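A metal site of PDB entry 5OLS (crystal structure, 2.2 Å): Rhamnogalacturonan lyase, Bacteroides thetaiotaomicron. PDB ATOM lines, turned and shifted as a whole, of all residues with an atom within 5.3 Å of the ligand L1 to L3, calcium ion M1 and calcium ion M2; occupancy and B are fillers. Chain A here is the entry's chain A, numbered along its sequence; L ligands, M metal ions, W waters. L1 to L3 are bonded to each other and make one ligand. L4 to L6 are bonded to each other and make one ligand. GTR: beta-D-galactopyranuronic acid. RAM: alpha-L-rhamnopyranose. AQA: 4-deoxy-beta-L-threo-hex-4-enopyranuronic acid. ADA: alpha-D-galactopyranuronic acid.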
ATOM      1  N   LYS A 189       4.493 -36.345   7.876  1.00  0.00           N
ATOM      2  CA  LYS A 189       3.518 -35.501   7.157  1.00  0.00           C
ATOM      3  C   LYS A 189       4.053 -35.083   5.782  1.00  0.00           C
ATOM      4  O   LYS A 189       3.315 -35.080   4.799  1.00  0.00           O
ATOM      5  CB  LYS A 189       3.154 -34.241   7.981  1.00  0.00           C
ATOM      6  CG  LYS A 189       2.084 -33.327   7.365  1.00  0.00           C
ATOM      7  CD  LYS A 189       0.680 -33.902   7.515  1.00  0.00           C
ATOM      8  CE  LYS A 189      -0.330 -33.295   6.526  1.00  0.00           C
ATOM      9  NZ  LYS A 189      -1.103 -32.137   7.041  1.00  0.00           N
ATOM     10  N   GLY A 191       4.961 -32.049   5.100  1.00  0.00           N
ATOM     11  CA  GLY A 191       4.329 -30.756   4.861  1.00  0.00           C
ATOM     12  C   GLY A 191       5.250 -29.595   4.484  1.00  0.00           C
ATOM     13  O   GLY A 191       4.767 -28.478   4.247  1.00  0.00           O
ATOM     14  N   ASN A 192       6.555 -29.838   4.452  1.00  0.00           N
ATOM     15  CA  ASN A 192       7.557 -28.811   4.153  1.00  0.00           C
ATOM     16  C   ASN A 192       8.320 -29.053   2.842  1.00  0.00           C
ATOM     17  O   ASN A 192       9.124 -28.202   2.433  1.00  0.00           O
ATOM     18  CB  ASN A 192       8.537 -28.719   5.323  1.00  0.00           C
ATOM     19  CG  ASN A 192       7.899 -28.154   6.586  1.00  0.00           C
ATOM     20  OD1 ASN A 192       6.843 -27.548   6.555  1.00  0.00           O
ATOM     21  ND2 ASN A 192       8.572 -28.342   7.718  1.00  0.00           N
ATOM     22  N   ASP A 194       8.422 -29.058  -0.818  1.00  0.00           N
ATOM     23  CA  ASP A 194       7.995 -28.597  -2.131  1.00  0.00           C
ATOM     24  C   ASP A 194       9.008 -28.915  -3.224  1.00  0.00           C
ATOM     25  O   ASP A 194      10.214 -29.120  -2.961  1.00  0.00           O
ATOM     26  CB  ASP A 194       7.779 -27.068  -2.142  1.00  0.00           C
ATOM     27  CG  ASP A 194       6.621 -26.605  -1.253  1.00  0.00           C
ATOM     28  OD1 ASP A 194       5.719 -27.401  -0.897  1.00  0.00           O
ATOM     29  OD2 ASP A 194       6.597 -25.401  -0.897  1.00  0.00           O
ATOM     30  N   HIS A 199      10.311 -17.721  -1.989  1.00  0.00           N
ATOM     31  CA  HIS A 199       9.987 -17.129  -0.677  1.00  0.00           C
ATOM     32  C   HIS A 199      10.949 -15.981  -0.341  1.00  0.00           C
ATOM     33  O   HIS A 199      11.588 -15.956   0.729  1.00  0.00           O
ATOM     34  CB  HIS A 199      10.018 -18.195   0.414  1.00  0.00           C
ATOM     35  CG  HIS A 199       9.308 -19.458   0.034  1.00  0.00           C
ATOM     36  ND1 HIS A 199       7.962 -19.496  -0.211  1.00  0.00           N
ATOM     37  CD2 HIS A 199       9.776 -20.702  -0.173  1.00  0.00           C
ATOM     38  CE1 HIS A 199       7.617 -20.725  -0.540  1.00  0.00           C
ATOM     39  NE2 HIS A 199       8.700 -21.482  -0.523  1.00  0.00           N
ATOM     40  N   ASP A 225       4.443 -32.121  -0.308  1.00  0.00           N
ATOM     41  CA  ASP A 225       3.621 -30.931  -0.060  1.00  0.00           C
ATOM     42  C   ASP A 225       3.064 -30.319  -1.378  1.00  0.00           C
ATOM     43  O   ASP A 225       2.011 -30.760  -1.887  1.00  0.00           O
ATOM     44  CB  ASP A 225       4.365 -29.923   0.820  1.00  0.00           C
ATOM     45  CG  ASP A 225       3.455 -28.845   1.400  1.00  0.00           C
ATOM     46  OD1 ASP A 225       2.414 -29.200   2.009  1.00  0.00           O
ATOM     47  OD2 ASP A 225       3.812 -27.627   1.297  1.00  0.00           O
ATOM     48  N   ASP A 226       3.757 -29.334  -1.947  1.00  0.00           N
ATOM     49  CA  ASP A 226       3.312 -28.685  -3.166  1.00  0.00           C
ATOM     50  C   ASP A 226       4.331 -28.912  -4.260  1.00  0.00           C
ATOM     51  O   ASP A 226       5.481 -29.324  -4.004  1.00  0.00           O
ATOM     52  CB  ASP A 226       3.108 -27.198  -2.921  1.00  0.00           C
ATOM     53  CG  ASP A 226       2.113 -26.924  -1.806  1.00  0.00           C
ATOM     54  OD1 ASP A 226       1.058 -27.594  -1.717  1.00  0.00           O
ATOM     55  OD2 ASP A 226       2.359 -25.997  -1.030  1.00  0.00           O
ATOM     56  N   ASP A 229       5.355 -23.191  -4.909  1.00  0.00           N
ATOM     57  CA  ASP A 229       4.840 -22.452  -3.755  1.00  0.00           C
ATOM     58  C   ASP A 229       5.542 -21.091  -3.665  1.00  0.00           C
ATOM     59  O   ASP A 229       6.781 -21.036  -3.586  1.00  0.00           O
ATOM     60  CB  ASP A 229       5.092 -23.292  -2.500  1.00  0.00           C
ATOM     61  CG  ASP A 229       4.568 -22.658  -1.212  1.00  0.00           C
ATOM     62  OD1 ASP A 229       4.151 -21.479  -1.222  1.00  0.00           O
ATOM     63  OD2 ASP A 229       4.600 -23.379  -0.174  1.00  0.00           O
ATOM     64  N   ILE A 231       4.568 -18.618  -1.210  1.00  0.00           N
ATOM     65  CA  ILE A 231       4.140 -18.001   0.026  1.00  0.00           C
ATOM     66  C   ILE A 231       5.301 -17.186   0.567  1.00  0.00           C
ATOM     67  O   ILE A 231       6.459 -17.525   0.323  1.00  0.00           O
ATOM     68  CB  ILE A 231       3.650 -19.048   1.065  1.00  0.00           C
ATOM     69  CG1 ILE A 231       2.620 -18.410   2.008  1.00  0.00           C
ATOM     70  CG2 ILE A 231       4.826 -19.667   1.836  1.00  0.00           C
ATOM     71  CD1 ILE A 231       2.117 -19.325   3.110  1.00  0.00           C
ATOM     72  N   ASP A 259      -0.065 -30.501   1.494  1.00  0.00           N
ATOM     73  CA  ASP A 259      -1.180 -29.656   1.028  1.00  0.00           C
ATOM     74  C   ASP A 259      -1.672 -29.922  -0.375  1.00  0.00           C
ATOM     75  O   ASP A 259      -2.796 -29.541  -0.723  1.00  0.00           O
ATOM     76  CB  ASP A 259      -0.814 -28.176   1.147  1.00  0.00           C
ATOM     77  CG  ASP A 259      -0.436 -27.790   2.558  1.00  0.00           C
ATOM     78  OD1 ASP A 259      -0.788 -28.524   3.484  1.00  0.00           O
ATOM     79  OD2 ASP A 259       0.242 -26.772   2.741  1.00  0.00           O
ATOM     80  N   GLY A 267       0.360 -15.632  -1.030  1.00  0.00           N
ATOM     81  CA  GLY A 267      -0.040 -15.846   0.345  1.00  0.00           C
ATOM     82  C   GLY A 267       0.990 -15.380   1.342  1.00  0.00           C
ATOM     83  O   GLY A 267       2.191 -15.384   1.060  1.00  0.00           O
ATOM     84  N   GLY A 269       0.096 -16.418   4.757  1.00  0.00           N
ATOM     85  CA  GLY A 269      -0.455 -17.175   5.862  1.00  0.00           C
ATOM     86  C   GLY A 269      -1.736 -16.581   6.417  1.00  0.00           C
ATOM     87  O   GLY A 269      -2.045 -15.400   6.225  1.00  0.00           O
ATOM     88  N   MET A 270      -2.450 -17.427   7.137  1.00  0.00           N
ATOM     89  CA  MET A 270      -3.651 -17.044   7.850  1.00  0.00           C
ATOM     90  C   MET A 270      -3.411 -17.335   9.336  1.00  0.00           C
ATOM     91  O   MET A 270      -4.208 -18.005   9.981  1.00  0.00           O
ATOM     92  CB  MET A 270      -4.843 -17.840   7.321  1.00  0.00           C
ATOM     93  CG  MET A 270      -5.139 -17.596   5.852  1.00  0.00           C
ATOM     94  SD  MET A 270      -5.940 -16.011   5.605  1.00  0.00           S
ATOM     95  CE  MET A 270      -7.623 -16.452   6.016  1.00  0.00           C
ATOM     96  N   ARG A 296      -3.226 -33.336  -5.028  1.00  0.00           N
ATOM     97  CA  ARG A 296      -4.168 -33.854  -4.046  1.00  0.00           C
ATOM     98  C   ARG A 296      -5.410 -32.966  -3.909  1.00  0.00           C
ATOM     99  O   ARG A 296      -6.529 -33.485  -3.899  1.00  0.00           O
ATOM    100  CB  ARG A 296      -3.536 -34.080  -2.666  1.00  0.00           C
ATOM    101  CG  ARG A 296      -4.389 -34.925  -1.737  1.00  0.00           C
ATOM    102  CD  ARG A 296      -3.634 -35.369  -0.483  1.00  0.00           C
ATOM    103  NE  ARG A 296      -3.459 -34.290   0.492  1.00  0.00           N
ATOM    104  CZ  ARG A 296      -4.421 -33.807   1.287  1.00  0.00           C
ATOM    105  NH1 ARG A 296      -4.136 -32.816   2.125  1.00  0.00           N
ATOM    106  NH2 ARG A 296      -5.666 -34.294   1.252  1.00  0.00           N
ATOM    107  N   LEU A 297      -5.222 -31.652  -3.829  1.00  0.00           N
ATOM    108  CA  LEU A 297      -6.308 -30.742  -3.439  1.00  0.00           C
ATOM    109  C   LEU A 297      -6.592 -29.623  -4.422  1.00  0.00           C
ATOM    110  O   LEU A 297      -7.756 -29.352  -4.708  1.00  0.00           O
ATOM    111  CB  LEU A 297      -6.041 -30.138  -2.049  1.00  0.00           C
ATOM    112  CG  LEU A 297      -6.337 -31.047  -0.850  1.00  0.00           C
ATOM    113  CD1 LEU A 297      -5.934 -30.397   0.475  1.00  0.00           C
ATOM    114  CD2 LEU A 297      -7.816 -31.445  -0.804  1.00  0.00           C
ATOM    115  N   ARG A 298      -5.559 -28.951  -4.913  1.00  0.00           N
ATOM    116  CA  ARG A 298      -5.758 -27.767  -5.739  1.00  0.00           C
ATOM    117  C   ARG A 298      -4.691 -27.651  -6.855  1.00  0.00           C
ATOM    118  O   ARG A 298      -3.574 -28.179  -6.742  1.00  0.00           O
ATOM    119  CB  ARG A 298      -5.777 -26.499  -4.876  1.00  0.00           C
ATOM    120  CG  ARG A 298      -6.575 -26.546  -3.565  1.00  0.00           C
ATOM    121  CD  ARG A 298      -6.395 -25.234  -2.798  1.00  0.00           C
ATOM    122  NE  ARG A 298      -7.278 -25.048  -1.649  1.00  0.00           N
ATOM    123  CZ  ARG A 298      -7.059 -25.501  -0.407  1.00  0.00           C
ATOM    124  NH1 ARG A 298      -6.001 -26.247  -0.101  1.00  0.00           N
ATOM    125  NH2 ARG A 298      -7.932 -25.227   0.549  1.00  0.00           N
ATOM    126  N   TYR A 301      -3.722 -21.739  -7.471  1.00  0.00           N
ATOM    127  CA  TYR A 301      -4.249 -21.283  -6.181  1.00  0.00           C
ATOM    128  C   TYR A 301      -3.589 -19.988  -5.702  1.00  0.00           C
ATOM    129  O   TYR A 301      -2.367 -19.891  -5.644  1.00  0.00           O
ATOM    130  CB  TYR A 301      -4.010 -22.395  -5.161  1.00  0.00           C
ATOM    131  CG  TYR A 301      -4.567 -22.213  -3.755  1.00  0.00           C
ATOM    132  CD1 TYR A 301      -5.775 -21.564  -3.501  1.00  0.00           C
ATOM    133  CD2 TYR A 301      -3.887 -22.762  -2.660  1.00  0.00           C
ATOM    134  CE1 TYR A 301      -6.285 -21.435  -2.201  1.00  0.00           C
ATOM    135  CE2 TYR A 301      -4.390 -22.651  -1.365  1.00  0.00           C
ATOM    136  CZ  TYR A 301      -5.587 -21.981  -1.133  1.00  0.00           C
ATOM    137  OH  TYR A 301      -6.068 -21.874   0.164  1.00  0.00           O
ATOM    138  N   ASN A 303      -3.940 -18.704  -2.716  1.00  0.00           N
ATOM    139  CA  ASN A 303      -3.329 -19.102  -1.464  1.00  0.00           C
ATOM    140  C   ASN A 303      -3.372 -17.953  -0.442  1.00  0.00           C
ATOM    141  O   ASN A 303      -2.385 -17.682   0.200  1.00  0.00           O
ATOM    142  CB  ASN A 303      -1.881 -19.573  -1.718  1.00  0.00           C
ATOM    143  CG  ASN A 303      -1.308 -20.395  -0.576  1.00  0.00           C
ATOM    144  OD1 ASN A 303      -1.982 -21.265  -0.040  1.00  0.00           O
ATOM    145  ND2 ASN A 303      -0.054 -20.125  -0.215  1.00  0.00           N
ATOM    146  N   HIS A 304      -4.526 -17.299  -0.336  1.00  0.00           N
ATOM    147  CA  HIS A 304      -4.732 -16.207   0.634  1.00  0.00           C
ATOM    148  C   HIS A 304      -3.823 -14.986   0.382  1.00  0.00           C
ATOM    149  O   HIS A 304      -3.345 -14.346   1.320  1.00  0.00           O
ATOM    150  CB  HIS A 304      -4.596 -16.736   2.081  1.00  0.00           C
ATOM    151  CG  HIS A 304      -5.223 -18.076   2.304  1.00  0.00           C
ATOM    152  ND1 HIS A 304      -6.560 -18.228   2.613  1.00  0.00           N
ATOM    153  CD2 HIS A 304      -4.705 -19.325   2.223  1.00  0.00           C
ATOM    154  CE1 HIS A 304      -6.835 -19.518   2.728  1.00  0.00           C
ATOM    155  NE2 HIS A 304      -5.720 -20.206   2.495  1.00  0.00           N
HETATM  156  C1  GTR L   1      -5.672 -27.608   4.035  1.00  0.00           C
HETATM  157  C2  GTR L   1      -4.308 -27.719   4.695  1.00  0.00           C
HETATM  158  C3  GTR L   1      -4.207 -26.598   5.735  1.00  0.00           C
HETATM  159  C4  GTR L   1      -4.374 -25.234   5.063  1.00  0.00           C
HETATM  160  C5  GTR L   1      -5.624 -25.207   4.139  1.00  0.00           C
HETATM  161  C6  GTR L   1      -5.689 -23.947   3.301  1.00  0.00           C
HETATM  162  O1  GTR L   1      -5.871 -28.743   3.196  1.00  0.00           O
HETATM  163  O2  GTR L   1      -4.078 -29.009   5.264  1.00  0.00           O
HETATM  164  O3  GTR L   1      -2.921 -26.691   6.385  1.00  0.00           O
HETATM  165  O4  GTR L   1      -3.103 -25.055   4.363  1.00  0.00           O
HETATM  166  O5  GTR L   1      -5.680 -26.373   3.286  1.00  0.00           O
HETATM  167  O6A GTR L   1      -5.271 -24.002   2.127  1.00  0.00           O
HETATM  168  O6B GTR L   1      -6.162 -22.887   3.777  1.00  0.00           O
HETATM  169  C1  RAM L   2      -2.532 -23.714   4.259  1.00  0.00           C
HETATM  170  C2  RAM L   2      -1.114 -23.614   3.690  1.00  0.00           C
HETATM  171  C3  RAM L   2      -1.222 -22.330   2.863  1.00  0.00           C
HETATM  172  C4  RAM L   2      -1.525 -21.149   3.779  1.00  0.00           C
HETATM  173  C5  RAM L   2      -2.823 -21.408   4.576  1.00  0.00           C
HETATM  174  C6  RAM L   2      -3.115 -20.343   5.605  1.00  0.00           C
HETATM  175  O2  RAM L   2      -0.131 -23.520   4.775  1.00  0.00           O
HETATM  176  O3  RAM L   2      -0.046 -22.122   2.089  1.00  0.00           O
HETATM  177  O4  RAM L   2      -1.592 -19.939   2.999  1.00  0.00           O
HETATM  178  O5  RAM L   2      -2.795 -22.686   5.228  1.00  0.00           O
HETATM  179  O6A AQA L   3       4.045 -22.845   2.375  1.00  0.00           O
HETATM  180  C6  AQA L   3       3.285 -23.859   2.759  1.00  0.00           C
HETATM  181  O6B AQA L   3       3.186 -24.840   2.015  1.00  0.00           O
HETATM  182  C5  AQA L   3       2.660 -23.838   3.934  1.00  0.00           C
HETATM  183  O5  AQA L   3       1.823 -24.974   4.293  1.00  0.00           O
HETATM  184  C4  AQA L   3       2.782 -22.807   4.807  1.00  0.00           C
HETATM  185  C3  AQA L   3       2.203 -22.887   6.215  1.00  0.00           C
HETATM  186  O3  AQA L   3       3.263 -22.740   7.173  1.00  0.00           O
HETATM  187  C2  AQA L   3       1.474 -24.207   6.468  1.00  0.00           C
HETATM  188  O2  AQA L   3       0.581 -24.026   7.581  1.00  0.00           O
HETATM  189  C1  AQA L   3       0.754 -24.635   5.189  1.00  0.00           C
HETATM  190  C1  RAM L   4       6.388 -22.225   5.952  1.00  0.00           C
HETATM  191  C2  RAM L   4       7.587 -22.510   6.864  1.00  0.00           C
HETATM  192  C3  RAM L   4       8.410 -23.621   6.245  1.00  0.00           C
HETATM  193  C4  RAM L   4       8.745 -23.353   4.779  1.00  0.00           C
HETATM  194  C5  RAM L   4       7.526 -22.946   3.959  1.00  0.00           C
HETATM  195  C6  RAM L   4       7.915 -22.457   2.569  1.00  0.00           C
HETATM  196  O1  RAM L   4       5.544 -23.378   5.917  1.00  0.00           O
HETATM  197  O2  RAM L   4       8.391 -21.325   6.967  1.00  0.00           O
HETATM  198  O3  RAM L   4       9.619 -23.799   6.981  1.00  0.00           O
HETATM  199  O4  RAM L   4       9.312 -24.543   4.223  1.00  0.00           O
HETATM  200  O5  RAM L   4       6.834 -21.888   4.628  1.00  0.00           O
HETATM  201  C1  ADA L   5       8.664 -20.837   8.307  1.00  0.00           C
HETATM  202  C2  ADA L   5       8.939 -19.343   8.208  1.00  0.00           C
HETATM  203  C3  ADA L   5      10.234 -19.073   7.447  1.00  0.00           C
HETATM  204  C4  ADA L   5      11.411 -19.837   8.028  1.00  0.00           C
HETATM  205  C5  ADA L   5      10.995 -21.311   8.182  1.00  0.00           C
HETATM  206  C6  ADA L   5      12.045 -22.235   8.726  1.00  0.00           C
HETATM  207  O2  ADA L   5       7.848 -18.708   7.535  1.00  0.00           O
HETATM  208  O3  ADA L   5      10.488 -17.660   7.499  1.00  0.00           O
HETATM  209  O4  ADA L   5      11.702 -19.194   9.264  1.00  0.00           O
HETATM  210  O5  ADA L   5       9.798 -21.419   8.964  1.00  0.00           O
HETATM  211  O6B ADA L   5      11.827 -22.790   9.826  1.00  0.00           O
HETATM  212  O6A ADA L   5      13.069 -22.451   8.046  1.00  0.00           O
HETATM  213  C1  RAM L   6      12.960 -18.594   9.470  1.00  0.00           C
HETATM  214  C2  RAM L   6      12.920 -17.340  10.270  1.00  0.00           C
HETATM  215  C3  RAM L   6      12.878 -17.749  11.724  1.00  0.00           C
HETATM  216  C4  RAM L   6      13.973 -18.767  12.030  1.00  0.00           C
HETATM  217  C5  RAM L   6      14.232 -19.823  10.921  1.00  0.00           C
HETATM  218  C6  RAM L   6      15.590 -20.482  11.155  1.00  0.00           C
HETATM  219  O2  RAM L   6      14.091 -16.541   9.990  1.00  0.00           O
HETATM  220  O3  RAM L   6      13.002 -16.562  12.511  1.00  0.00           O
HETATM  221  O4  RAM L   6      13.564 -19.461  13.216  1.00  0.00           O
HETATM  222  O5  RAM L   6      14.143 -19.323   9.559  1.00  0.00           O
HETATM  223 CA    CA M   1       4.484 -25.813   0.278  1.00  0.00          CA
HETATM  224 CA    CA M   2       2.847 -27.060   3.809  1.00  0.00          CA
HETATM  225  O   HOH W   1       0.709 -25.232   0.748  1.00  0.00           O
HETATM  226  O   HOH W   2       5.903 -25.795   2.123  1.00  0.00           O
HETATM  227  O   HOH W   3       2.224 -27.881   5.986  1.00  0.00           O
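Water W1 bridges OD1 of Asp 226 (3.4 Å) and O3 of RAM L2 (3.5 Å).
O3 of AQA L3 is in hydrogen-bond range of O1 of RAM L4, 2.7 Å away.
Within 4 Å of calcium ion M1: Asp 194, Asp 225, Asp 226 and Asp 229. Along chain A the residues within 4 Å of calcium ion M1 span positions 194 to 229.
Calcium ion M2 is bound by O5 of AQA L3 (2.4 Å). Water W3 is bound to calcium ion M2 (2.4 Å). O of Gly 191 is bound to calcium ion M2 (2.4 Å). The side-chain carboxylate (OD2) of Asp 225 is bound to calcium ion M2, 2.8 Å away. The side-chain carboxylate (OD1) of Asp 225 is bound to calcium ion M2 (2.8 Å). The side-chain carboxylate (OD2) of Asp 259 is bound to calcium ion M2, at 2.8 Å. Calcium ion M2 is bound by O6B of AQA L3.
The side-chain carboxylate (OD1) of Asp 229 sits at hydrogen-bond distance from the backbone NH (N) of Ile 231, at 2.9 Å. A ring nitrogen (ND1) of His 304 lies close to the side-chain sulfur (SD) of Met 270 (3.8 Å). ND1 of His 199 is in hydrogen-bond range of O of Ile 231 (2.5 Å). OH of Tyr 301 sits at hydrogen-bond distance from NE2 of His 304 (2.9 Å).
Residues that only touch the ligand L1 to L3: Ile 231 (3.3 Å), Met 270 (3.4 Å) and Leu 297 (3.2 Å). Hydrophobic or aromatic side chains within 4 Å of the ligand L1 to L3: Ile 231, Met 270, Leu 297, Tyr 301 and His 304. The nearest printed residue that does not touch the ligand L1 to L3 is Gly 269 (4.1 Å).
OD2 of Asp 225 binds calcium ion M1 (2.2 Å). Water W2 binds calcium ion M1 (2.3 Å). The side-chain carboxylate (OD1) of Asp 194 binds calcium ion M1, 2.3 Å away. Calcium ion M1 is bound by O6B of AQA L3, at 2.4 Å. Calcium ion M1 is bound by the side-chain carboxylate (OD2) of Asp 194, 2.5 Å away. Calcium ion M1 is bound by OD2 of Asp 229, 2.5 Å away. Calcium ion M1 is bound by OD2 of Asp 226 (2.5 Å).
An oxygen (O6B) of GTR L1 sits at hydrogen-bond distance from a ring nitrogen (NE2) of His 304. An oxygen (O6A) of GTR L1 is in hydrogen-bond range of the side-chain hydroxyl (OH) of Tyr 301 (3.0 Å). An oxygen (O3) of RAM L2 lies within hydrogen-bond range of the side-chain amide oxygen of Asn 303 (3.0 Å). An oxygen (O6A) of GTR L1 lies within salt-bridge range of the guanidinium group of Arg 298 (3.2 Å).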
